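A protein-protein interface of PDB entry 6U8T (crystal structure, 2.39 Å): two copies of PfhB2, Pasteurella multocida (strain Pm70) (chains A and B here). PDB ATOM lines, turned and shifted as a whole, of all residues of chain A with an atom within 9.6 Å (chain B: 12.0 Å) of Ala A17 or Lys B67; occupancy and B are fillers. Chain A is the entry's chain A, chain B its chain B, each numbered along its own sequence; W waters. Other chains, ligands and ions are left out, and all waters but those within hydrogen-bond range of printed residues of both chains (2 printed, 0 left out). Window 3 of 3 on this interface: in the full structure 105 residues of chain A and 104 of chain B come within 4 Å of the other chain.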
ATOM      1  N   MET A   2      -9.058   0.654 -30.190  1.00  0.00           N
ATOM      2  CA  MET A   2     -10.073   1.195 -29.294  1.00  0.00           C
ATOM      3  C   MET A   2      -9.526   2.375 -28.496  1.00  0.00           C
ATOM      4  O   MET A   2     -10.132   2.833 -27.515  1.00  0.00           O
ATOM      5  CB  MET A   2     -10.552   0.065 -28.387  1.00  0.00           C
ATOM      6  CG  MET A   2     -11.602  -0.790 -29.067  1.00  0.00           C
ATOM      7  SD  MET A   2     -12.286  -2.139 -27.832  1.00  0.00           S
ATOM      8  CE  MET A   2     -14.132  -2.306 -27.307  1.00  0.00           C
ATOM      9  N   SER A  13     -16.272  -1.526 -22.599  1.00  0.00           N
ATOM     10  CA  SER A  13     -16.891  -2.422 -21.597  1.00  0.00           C
ATOM     11  C   SER A  13     -16.003  -3.642 -21.382  1.00  0.00           C
ATOM     12  O   SER A  13     -16.142  -4.273 -20.332  1.00  0.00           O
ATOM     13  CB  SER A  13     -18.268  -2.892 -22.005  1.00  0.00           C
ATOM     14  OG  SER A  13     -19.015  -1.881 -22.673  1.00  0.00           O
ATOM     15  N   PHE A  14     -15.219  -4.035 -22.383  1.00  0.00           N
ATOM     16  CA  PHE A  14     -14.385  -5.257 -22.360  1.00  0.00           C
ATOM     17  C   PHE A  14     -13.278  -5.079 -23.395  1.00  0.00           C
ATOM     18  O   PHE A  14     -13.526  -4.588 -24.528  1.00  0.00           O
ATOM     19  CB  PHE A  14     -15.198  -6.518 -22.673  1.00  0.00           C
ATOM     20  CG  PHE A  14     -14.389  -7.799 -22.641  1.00  0.00           C
ATOM     21  CD1 PHE A  14     -13.959  -8.362 -21.439  1.00  0.00           C
ATOM     22  CD2 PHE A  14     -14.025  -8.428 -23.823  1.00  0.00           C
ATOM     23  CE1 PHE A  14     -13.187  -9.524 -21.426  1.00  0.00           C
ATOM     24  CE2 PHE A  14     -13.287  -9.611 -23.813  1.00  0.00           C
ATOM     25  CZ  PHE A  14     -12.860 -10.157 -22.611  1.00  0.00           C
ATOM     26  N   LYS A  15     -12.074  -5.480 -23.036  1.00  0.00           N
ATOM     27  CA  LYS A  15     -10.907  -5.425 -23.945  1.00  0.00           C
ATOM     28  C   LYS A  15     -10.234  -6.796 -23.898  1.00  0.00           C
ATOM     29  O   LYS A  15      -9.901  -7.268 -22.772  1.00  0.00           O
ATOM     30  CB  LYS A  15     -10.007  -4.262 -23.513  1.00  0.00           C
ATOM     31  CG  LYS A  15      -8.721  -4.116 -24.315  1.00  0.00           C
ATOM     32  CD  LYS A  15      -7.817  -3.053 -23.770  1.00  0.00           C
ATOM     33  CE  LYS A  15      -6.967  -2.362 -24.825  1.00  0.00           C
ATOM     34  NZ  LYS A  15      -5.615  -2.020 -24.291  1.00  0.00           N
ATOM     35  N   TYR A  16     -10.092  -7.451 -25.044  1.00  0.00           N
ATOM     36  CA  TYR A  16      -9.407  -8.786 -25.079  1.00  0.00           C
ATOM     37  C   TYR A  16      -7.933  -8.568 -24.790  1.00  0.00           C
ATOM     38  O   TYR A  16      -7.284  -7.705 -25.428  1.00  0.00           O
ATOM     39  CB  TYR A  16      -9.513  -9.477 -26.426  1.00  0.00           C
ATOM     40  CG  TYR A  16     -10.781 -10.216 -26.727  1.00  0.00           C
ATOM     41  CD1 TYR A  16     -11.850  -9.555 -27.284  1.00  0.00           C
ATOM     42  CD2 TYR A  16     -10.837 -11.599 -26.636  1.00  0.00           C
ATOM     43  CE1 TYR A  16     -13.016 -10.225 -27.621  1.00  0.00           C
ATOM     44  CE2 TYR A  16     -11.983 -12.296 -27.015  1.00  0.00           C
ATOM     45  CZ  TYR A  16     -13.079 -11.601 -27.499  1.00  0.00           C
ATOM     46  OH  TYR A  16     -14.212 -12.273 -27.866  1.00  0.00           O
ATOM     47  N   ALA A  17      -7.416  -9.369 -23.872  1.00  0.00           N
ATOM     48  CA  ALA A  17      -6.012  -9.336 -23.419  1.00  0.00           C
ATOM     49  C   ALA A  17      -5.127  -9.590 -24.627  1.00  0.00           C
ATOM     50  O   ALA A  17      -4.138  -8.862 -24.780  1.00  0.00           O
ATOM     51  CB  ALA A  17      -5.806 -10.325 -22.297  1.00  0.00           C
ATOM     52  N   GLN A  18      -5.484 -10.559 -25.460  1.00  0.00           N
ATOM     53  CA  GLN A  18      -4.752 -10.842 -26.722  1.00  0.00           C
ATOM     54  C   GLN A  18      -5.693 -10.475 -27.864  1.00  0.00           C
ATOM     55  O   GLN A  18      -6.776 -11.157 -28.034  1.00  0.00           O
ATOM     56  CB  GLN A  18      -4.322 -12.301 -26.839  1.00  0.00           C
ATOM     57  CG  GLN A  18      -2.996 -12.589 -26.166  1.00  0.00           C
ATOM     58  CD  GLN A  18      -3.213 -13.155 -24.791  1.00  0.00           C
ATOM     59  OE1 GLN A  18      -2.409 -12.950 -23.888  1.00  0.00           O
ATOM     60  NE2 GLN A  18      -4.333 -13.845 -24.629  1.00  0.00           N
ATOM     61  N   SER A  19      -5.345  -9.396 -28.555  1.00  0.00           N
ATOM     62  CA  SER A  19      -6.177  -8.831 -29.642  1.00  0.00           C
ATOM     63  C   SER A  19      -5.911  -9.657 -30.901  1.00  0.00           C
ATOM     64  O   SER A  19      -4.806  -9.552 -31.421  1.00  0.00           O
ATOM     65  CB  SER A  19      -5.879  -7.369 -29.807  1.00  0.00           C
ATOM     66  OG  SER A  19      -6.512  -6.846 -30.950  1.00  0.00           O
ATOM     67  N   LYS A  20      -6.871 -10.441 -31.367  1.00  0.00           N
ATOM     68  CA  LYS A  20      -6.745 -11.082 -32.704  1.00  0.00           C
ATOM     69  C   LYS A  20      -6.750 -10.013 -33.823  1.00  0.00           C
ATOM     70  O   LYS A  20      -6.255 -10.304 -34.921  1.00  0.00           O
ATOM     71  CB  LYS A  20      -7.821 -12.157 -32.898  1.00  0.00           C
ATOM     72  CG  LYS A  20      -7.695 -13.317 -31.942  1.00  0.00           C
ATOM     73  CD  LYS A  20      -6.326 -13.959 -31.924  1.00  0.00           C
ATOM     74  CE  LYS A  20      -6.098 -14.655 -30.591  1.00  0.00           C
ATOM     75  NZ  LYS A  20      -5.377 -15.941 -30.745  1.00  0.00           N
ATOM     76  N   GLY A  21      -7.265  -8.816 -33.540  1.00  0.00           N
ATOM     77  CA  GLY A  21      -7.213  -7.637 -34.425  1.00  0.00           C
ATOM     78  C   GLY A  21      -5.788  -7.184 -34.646  1.00  0.00           C
ATOM     79  O   GLY A  21      -5.430  -6.867 -35.808  1.00  0.00           O
ATOM     80  N   GLU A  22      -4.979  -7.163 -33.595  1.00  0.00           N
ATOM     81  CA  GLU A  22      -3.554  -6.751 -33.717  1.00  0.00           C
ATOM     82  C   GLU A  22      -2.788  -7.801 -34.529  1.00  0.00           C
ATOM     83  O   GLU A  22      -1.990  -7.405 -35.361  1.00  0.00           O
ATOM     84  CB  GLU A  22      -2.913  -6.493 -32.355  1.00  0.00           C
ATOM     85  CG  GLU A  22      -3.432  -5.222 -31.686  1.00  0.00           C
ATOM     86  CD  GLU A  22      -3.466  -3.964 -32.549  1.00  0.00           C
ATOM     87  OE1 GLU A  22      -2.475  -3.687 -33.276  1.00  0.00           O
ATOM     88  OE2 GLU A  22      -4.493  -3.254 -32.498  1.00  0.00           O
ATOM     89  N   VAL A  23      -3.070  -9.083 -34.327  1.00  0.00           N
ATOM     90  CA  VAL A  23      -2.540 -10.193 -35.171  1.00  0.00           C
ATOM     91  C   VAL A  23      -2.944  -9.935 -36.615  1.00  0.00           C
ATOM     92  O   VAL A  23      -2.094 -10.045 -37.475  1.00  0.00           O
ATOM     93  CB  VAL A  23      -2.997 -11.586 -34.679  1.00  0.00           C
ATOM     94  CG1 VAL A  23      -2.617 -12.690 -35.655  1.00  0.00           C
ATOM     95  CG2 VAL A  23      -2.473 -11.909 -33.273  1.00  0.00           C
ATOM     96  N   PRO A 177     -14.964  -9.332 -31.803  1.00  0.00           N
ATOM     97  CA  PRO A 177     -14.199 -10.367 -31.115  1.00  0.00           C
ATOM     98  C   PRO A 177     -12.681 -10.228 -31.283  1.00  0.00           C
ATOM     99  O   PRO A 177     -11.951 -10.907 -30.566  1.00  0.00           O
ATOM    100  CB  PRO A 177     -14.613 -11.700 -31.722  1.00  0.00           C
ATOM    101  CG  PRO A 177     -15.747 -11.385 -32.721  1.00  0.00           C
ATOM    102  CD  PRO A 177     -15.914  -9.877 -32.791  1.00  0.00           C
ATOM    103  N   ASN A 178     -12.251  -9.349 -32.182  1.00  0.00           N
ATOM    104  CA  ASN A 178     -10.826  -9.019 -32.449  1.00  0.00           C
ATOM    105  C   ASN A 178     -10.336  -7.936 -31.495  1.00  0.00           C
ATOM    106  O   ASN A 178      -9.114  -7.748 -31.465  1.00  0.00           O
ATOM    107  CB  ASN A 178     -10.612  -8.535 -33.893  1.00  0.00           C
ATOM    108  CG  ASN A 178     -10.384  -9.649 -34.894  1.00  0.00           C
ATOM    109  OD1 ASN A 178     -10.453 -10.842 -34.540  1.00  0.00           O
ATOM    110  ND2 ASN A 178     -10.151  -9.228 -36.149  1.00  0.00           N
ATOM    111  N   PHE A 179     -11.239  -7.213 -30.807  1.00  0.00           N
ATOM    112  CA  PHE A 179     -10.864  -6.081 -29.915  1.00  0.00           C
ATOM    113  C   PHE A 179     -11.627  -6.130 -28.588  1.00  0.00           C
ATOM    114  O   PHE A 179     -10.978  -6.116 -27.520  1.00  0.00           O
ATOM    115  CB  PHE A 179     -11.069  -4.757 -30.630  1.00  0.00           C
ATOM    116  CG  PHE A 179     -10.219  -4.602 -31.875  1.00  0.00           C
ATOM    117  CD1 PHE A 179      -8.873  -4.301 -31.777  1.00  0.00           C
ATOM    118  CD2 PHE A 179     -10.774  -4.748 -33.134  1.00  0.00           C
ATOM    119  CE1 PHE A 179      -8.093  -4.163 -32.909  1.00  0.00           C
ATOM    120  CE2 PHE A 179      -9.992  -4.597 -34.268  1.00  0.00           C
ATOM    121  CZ  PHE A 179      -8.650  -4.307 -34.152  1.00  0.00           C
ATOM    122  N   GLY A 180     -12.955  -6.194 -28.628  1.00  0.00           N
ATOM    123  CA  GLY A 180     -13.801  -6.283 -27.431  1.00  0.00           C
ATOM    124  C   GLY A 180     -15.136  -5.578 -27.608  1.00  0.00           C
ATOM    125  O   GLY A 180     -15.643  -5.571 -28.706  1.00  0.00           O
ATOM    126  N   GLN B  34     -10.126 -18.087 -37.914  1.00  0.00           N
ATOM    127  CA  GLN B  34     -10.462 -16.898 -37.106  1.00  0.00           C
ATOM    128  C   GLN B  34     -11.852 -16.363 -37.516  1.00  0.00           C
ATOM    129  O   GLN B  34     -12.553 -15.808 -36.663  1.00  0.00           O
ATOM    130  CB  GLN B  34      -9.337 -15.872 -37.231  1.00  0.00           C
ATOM    131  CG  GLN B  34      -9.271 -14.939 -36.033  1.00  0.00           C
ATOM    132  CD  GLN B  34      -9.011 -15.690 -34.753  1.00  0.00           C
ATOM    133  OE1 GLN B  34      -8.186 -16.579 -34.697  1.00  0.00           O
ATOM    134  NE2 GLN B  34      -9.693 -15.309 -33.695  1.00  0.00           N
ATOM    135  N   THR B  41     -18.273 -16.505 -31.733  1.00  0.00           N
ATOM    136  CA  THR B  41     -18.220 -15.594 -30.572  1.00  0.00           C
ATOM    137  C   THR B  41     -19.355 -14.566 -30.664  1.00  0.00           C
ATOM    138  O   THR B  41     -20.011 -14.359 -29.657  1.00  0.00           O
ATOM    139  CB  THR B  41     -16.901 -14.828 -30.447  1.00  0.00           C
ATOM    140  OG1 THR B  41     -15.813 -15.750 -30.417  1.00  0.00           O
ATOM    141  CG2 THR B  41     -16.905 -13.960 -29.191  1.00  0.00           C
ATOM    142  N   THR B  60     -22.591 -12.668 -17.489  1.00  0.00           N
ATOM    143  CA  THR B  60     -21.517 -12.139 -18.376  1.00  0.00           C
ATOM    144  C   THR B  60     -20.801 -13.326 -19.027  1.00  0.00           C
ATOM    145  O   THR B  60     -20.843 -14.433 -18.500  1.00  0.00           O
ATOM    146  CB  THR B  60     -20.626 -11.170 -17.598  1.00  0.00           C
ATOM    147  OG1 THR B  60     -19.637 -10.851 -18.569  1.00  0.00           O
ATOM    148  CG2 THR B  60     -20.025 -11.738 -16.336  1.00  0.00           C
ATOM    149  N   MET B  61     -20.214 -13.128 -20.212  1.00  0.00           N
ATOM    150  CA  MET B  61     -19.297 -14.119 -20.763  1.00  0.00           C
ATOM    151  C   MET B  61     -17.853 -13.819 -20.364  1.00  0.00           C
ATOM    152  O   MET B  61     -16.955 -14.608 -20.674  1.00  0.00           O
ATOM    153  CB  MET B  61     -19.257 -14.137 -22.288  1.00  0.00           C
ATOM    154  CG  MET B  61     -20.558 -14.027 -23.023  1.00  0.00           C
ATOM    155  SD  MET B  61     -20.080 -14.248 -24.934  1.00  0.00           S
ATOM    156  CE  MET B  61     -18.559 -13.194 -25.548  1.00  0.00           C
ATOM    157  N   TYR B  62     -17.646 -12.699 -19.660  1.00  0.00           N
ATOM    158  CA  TYR B  62     -16.332 -12.201 -19.301  1.00  0.00           C
ATOM    159  C   TYR B  62     -15.915 -12.738 -17.933  1.00  0.00           C
ATOM    160  O   TYR B  62     -16.735 -12.699 -17.009  1.00  0.00           O
ATOM    161  CB  TYR B  62     -16.331 -10.668 -19.374  1.00  0.00           C
ATOM    162  CG  TYR B  62     -16.814 -10.134 -20.713  1.00  0.00           C
ATOM    163  CD1 TYR B  62     -16.350 -10.665 -21.916  1.00  0.00           C
ATOM    164  CD2 TYR B  62     -17.746  -9.104 -20.781  1.00  0.00           C
ATOM    165  CE1 TYR B  62     -16.775 -10.167 -23.136  1.00  0.00           C
ATOM    166  CE2 TYR B  62     -18.167  -8.584 -21.987  1.00  0.00           C
ATOM    167  CZ  TYR B  62     -17.700  -9.137 -23.165  1.00  0.00           C
ATOM    168  OH  TYR B  62     -18.149  -8.708 -24.364  1.00  0.00           O
ATOM    169  N   GLU B  63     -14.675 -13.228 -17.835  1.00  0.00           N
ATOM    170  CA  GLU B  63     -14.071 -13.775 -16.586  1.00  0.00           C
ATOM    171  C   GLU B  63     -13.880 -12.622 -15.592  1.00  0.00           C
ATOM    172  O   GLU B  63     -13.138 -11.713 -15.917  1.00  0.00           O
ATOM    173  CB  GLU B  63     -12.748 -14.497 -16.904  1.00  0.00           C
ATOM    174  CG  GLU B  63     -12.211 -15.388 -15.774  1.00  0.00           C
ATOM    175  CD  GLU B  63     -13.269 -16.133 -14.977  1.00  0.00           C
ATOM    176  OE1 GLU B  63     -14.014 -16.941 -15.570  1.00  0.00           O
ATOM    177  OE2 GLU B  63     -13.376 -15.878 -13.752  1.00  0.00           O
ATOM    178  N   GLY B  64     -14.537 -12.670 -14.430  1.00  0.00           N
ATOM    179  CA  GLY B  64     -14.475 -11.635 -13.379  1.00  0.00           C
ATOM    180  C   GLY B  64     -13.056 -11.352 -12.932  1.00  0.00           C
ATOM    181  O   GLY B  64     -12.726 -10.191 -12.741  1.00  0.00           O
ATOM    182  N   GLY B  65     -12.247 -12.393 -12.754  1.00  0.00           N
ATOM    183  CA  GLY B  65     -10.974 -12.325 -12.005  1.00  0.00           C
ATOM    184  C   GLY B  65      -9.765 -12.483 -12.895  1.00  0.00           C
ATOM    185  O   GLY B  65      -8.653 -12.541 -12.372  1.00  0.00           O
ATOM    186  N   LYS B  66      -9.989 -12.527 -14.200  1.00  0.00           N
ATOM    187  CA  LYS B  66      -8.947 -12.659 -15.245  1.00  0.00           C
ATOM    188  C   LYS B  66      -9.234 -11.562 -16.278  1.00  0.00           C
ATOM    189  O   LYS B  66     -10.114 -11.789 -17.108  1.00  0.00           O
ATOM    190  CB  LYS B  66      -9.009 -14.085 -15.816  1.00  0.00           C
ATOM    191  CG  LYS B  66      -7.714 -14.609 -16.417  1.00  0.00           C
ATOM    192  CD  LYS B  66      -7.908 -15.729 -17.414  1.00  0.00           C
ATOM    193  CE  LYS B  66      -6.606 -16.086 -18.095  1.00  0.00           C
ATOM    194  NZ  LYS B  66      -6.567 -17.509 -18.492  1.00  0.00           N
ATOM    195  N   LYS B  67      -8.565 -10.409 -16.185  1.00  0.00           N
ATOM    196  CA  LYS B  67      -8.876  -9.211 -17.017  1.00  0.00           C
ATOM    197  C   LYS B  67      -8.612  -9.552 -18.493  1.00  0.00           C
ATOM    198  O   LYS B  67      -7.509 -10.032 -18.808  1.00  0.00           O
ATOM    199  CB  LYS B  67      -8.094  -7.970 -16.570  1.00  0.00           C
ATOM    200  CG  LYS B  67      -6.959  -7.540 -17.493  1.00  0.00           C
ATOM    201  CD  LYS B  67      -6.231  -6.287 -17.057  1.00  0.00           C
ATOM    202  CE  LYS B  67      -7.103  -5.048 -17.017  1.00  0.00           C
ATOM    203  NZ  LYS B  67      -7.057  -4.376 -15.687  1.00  0.00           N
ATOM    204  N   GLY B  68      -9.621  -9.358 -19.344  1.00  0.00           N
ATOM    205  CA  GLY B  68      -9.494  -9.399 -20.804  1.00  0.00           C
ATOM    206  C   GLY B  68      -9.610 -10.806 -21.346  1.00  0.00           C
ATOM    207  O   GLY B  68      -9.051 -11.059 -22.400  1.00  0.00           O
ATOM    208  N   HIS B  69     -10.324 -11.688 -20.638  1.00  0.00           N
ATOM    209  CA  HIS B  69     -10.529 -13.101 -21.049  1.00  0.00           C
ATOM    210  C   HIS B  69     -11.992 -13.483 -20.907  1.00  0.00           C
ATOM    211  O   HIS B  69     -12.676 -12.916 -20.031  1.00  0.00           O
ATOM    212  CB  HIS B  69      -9.641 -14.051 -20.258  1.00  0.00           C
ATOM    213  CG  HIS B  69      -8.189 -13.867 -20.503  1.00  0.00           C
ATOM    214  ND1 HIS B  69      -7.566 -14.393 -21.614  1.00  0.00           N
ATOM    215  CD2 HIS B  69      -7.232 -13.247 -19.780  1.00  0.00           C
ATOM    216  CE1 HIS B  69      -6.279 -14.074 -21.595  1.00  0.00           C
ATOM    217  NE2 HIS B  69      -6.034 -13.398 -20.434  1.00  0.00           N
ATOM    218  N   LEU B  70     -12.438 -14.416 -21.751  1.00  0.00           N
ATOM    219  CA  LEU B  70     -13.793 -15.003 -21.678  1.00  0.00           C
ATOM    220  C   LEU B  70     -13.749 -16.096 -20.613  1.00  0.00           C
ATOM    221  O   LEU B  70     -12.661 -16.589 -20.324  1.00  0.00           O
ATOM    222  CB  LEU B  70     -14.204 -15.546 -23.048  1.00  0.00           C
ATOM    223  CG  LEU B  70     -14.195 -14.575 -24.238  1.00  0.00           C
ATOM    224  CD1 LEU B  70     -14.896 -15.241 -25.422  1.00  0.00           C
ATOM    225  CD2 LEU B  70     -14.883 -13.245 -23.927  1.00  0.00           C
ATOM    226  N   LYS B  71     -14.884 -16.403 -19.982  1.00  0.00           N
ATOM    227  CA  LYS B  71     -15.015 -17.568 -19.078  1.00  0.00           C
ATOM    228  C   LYS B  71     -14.726 -18.830 -19.883  1.00  0.00           C
ATOM    229  O   LYS B  71     -15.064 -18.850 -21.122  1.00  0.00           O
ATOM    230  CB  LYS B  71     -16.442 -17.648 -18.563  1.00  0.00           C
ATOM    231  CG  LYS B  71     -16.817 -16.589 -17.543  1.00  0.00           C
ATOM    232  CD  LYS B  71     -18.281 -16.693 -17.192  1.00  0.00           C
ATOM    233  CE  LYS B  71     -18.693 -15.905 -15.960  1.00  0.00           C
ATOM    234  NZ  LYS B  71     -20.104 -16.243 -15.677  1.00  0.00           N
ATOM    235  N   GLN B  72     -14.174 -19.844 -19.214  1.00  0.00           N
ATOM    236  CA  GLN B  72     -13.762 -21.138 -19.810  1.00  0.00           C
ATOM    237  C   GLN B  72     -14.989 -21.841 -20.411  1.00  0.00           C
ATOM    238  O   GLN B  72     -14.841 -22.393 -21.502  1.00  0.00           O
ATOM    239  CB  GLN B  72     -13.049 -22.032 -18.795  1.00  0.00           C
ATOM    240  CG  GLN B  72     -12.322 -23.192 -19.442  1.00  0.00           C
ATOM    241  CD  GLN B  72     -11.347 -22.770 -20.523  1.00  0.00           C
ATOM    242  OE1 GLN B  72     -10.536 -21.866 -20.325  1.00  0.00           O
ATOM    243  NE2 GLN B  72     -11.433 -23.403 -21.693  1.00  0.00           N
ATOM    244  N   ILE B  75     -15.748 -20.231 -23.728  1.00  0.00           N
ATOM    245  CA  ILE B  75     -14.661 -20.618 -24.679  1.00  0.00           C
ATOM    246  C   ILE B  75     -14.980 -22.019 -25.236  1.00  0.00           C
ATOM    247  O   ILE B  75     -14.875 -22.217 -26.467  1.00  0.00           O
ATOM    248  CB  ILE B  75     -13.270 -20.558 -24.012  1.00  0.00           C
ATOM    249  CG1 ILE B  75     -12.793 -19.109 -23.867  1.00  0.00           C
ATOM    250  CG2 ILE B  75     -12.250 -21.386 -24.766  1.00  0.00           C
ATOM    251  CD1 ILE B  75     -11.799 -18.883 -22.707  1.00  0.00           C
HETATM  252  O   HOH W   1     -11.736 -13.295 -33.477  1.00  0.00           O
HETATM  253  O   HOH W   2     -13.439 -14.836 -28.884  1.00  0.00           O
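Lys A15 touches just one residue of chain B: Gly B68. Of the printed residues of chain B, Tyr A16 touches Thr B41, Gly B68 and Leu B70. Ala A17 touches three residues of chain B. Gln A18 touches one residue of chain B. No residue of chain B comes within 4 Å of Ser A19. Pro A177 touches none of the printed residues of chain B. Printed residues of chain A within 4 Å of Gln B34: Lys A20 (3.3 Å). Of the printed residues of chain A, Thr B41 touches Tyr A16 (3.4 Å). No residue of chain A comes within 4 Å of Gly B65. Lys B66 touches none of the printed residues of chain A. Of the printed residues of chain A, Lys B67 touches Ala A17. Gly B68 touches just these residues of chain A: Phe A14 (3.5 Å), Lys A15 (2.9 Å), Tyr A16 (3.5 Å) and Ala A17 (2.8 Å). Of the printed residues of chain A, His B69 touches Phe A14, Ala A17 and Gln A18. Of the printed residues of chain A, Leu B70 touches Phe A14 (3.9 Å) and Tyr A16 (3.9 Å). The nearest residue of chain A that does not touch Lys B67 is Lys A15 (5.0 Å).
Hydrophobic or aromatic side chains of chain A that line the printed part of chain B: Phe A14, Tyr A16 and Ala A17. Along chain A the printed residues that touch a printed residue of chain B span positions 14 to 20. Of the 16 printed residues of chain B, 7 touch a printed residue of chain A. Among the printed residues, 13 pairs touch across the chains.
The backbone NH (N) of Ala A17 sits at hydrogen-bond distance from the backbone carbonyl oxygen (O) of Gly B68, 2.8 Å away.
Water W2 bridges the side-chain hydroxyl of Tyr A16 (2.9 Å) and the side-chain hydroxyl of Thr B41 (3.0 Å). Water W1 bridges the side-chain amide nitrogen (NE2) of Gln B34 (2.9 Å) and the side-chain amide oxygen (OD1) of Asn A178 (3.0 Å).
No position is printed for both chains.
Among the printed residues, merely in contact across the chains: Phe A14 with Tyr B62 (3.3 Å), Phe A14 with Gly B68 (3.5 Å), Phe A14 with His B69 (3.6 Å), Phe A14 with Leu B70 (3.9 Å), Lys A15 with Gly B68 (2.9 Å), Tyr A16 with Thr B41 (3.4 Å), Tyr A16 with Gly B68 (3.5 Å), Tyr A16 with Leu B70 (3.9 Å), Ala A17 with Lys B67 (3.9 Å), Ala A17 with His B69 (3.6 Å), Gln A18 with His B69 (3.6 Å) and Lys A20 with Gln B34 (3.3 Å).
N of Tyr A16 is in hydrogen-bond range of O of Phe A179, at 2.9 Å. OG1 of Thr B60 is in hydrogen-bond range of N of Tyr B62 (2.9 Å). The backbone NH (N) of Glu B63 sits at hydrogen-bond distance from the backbone carbonyl oxygen (O) of His B69 (3.0 Å).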
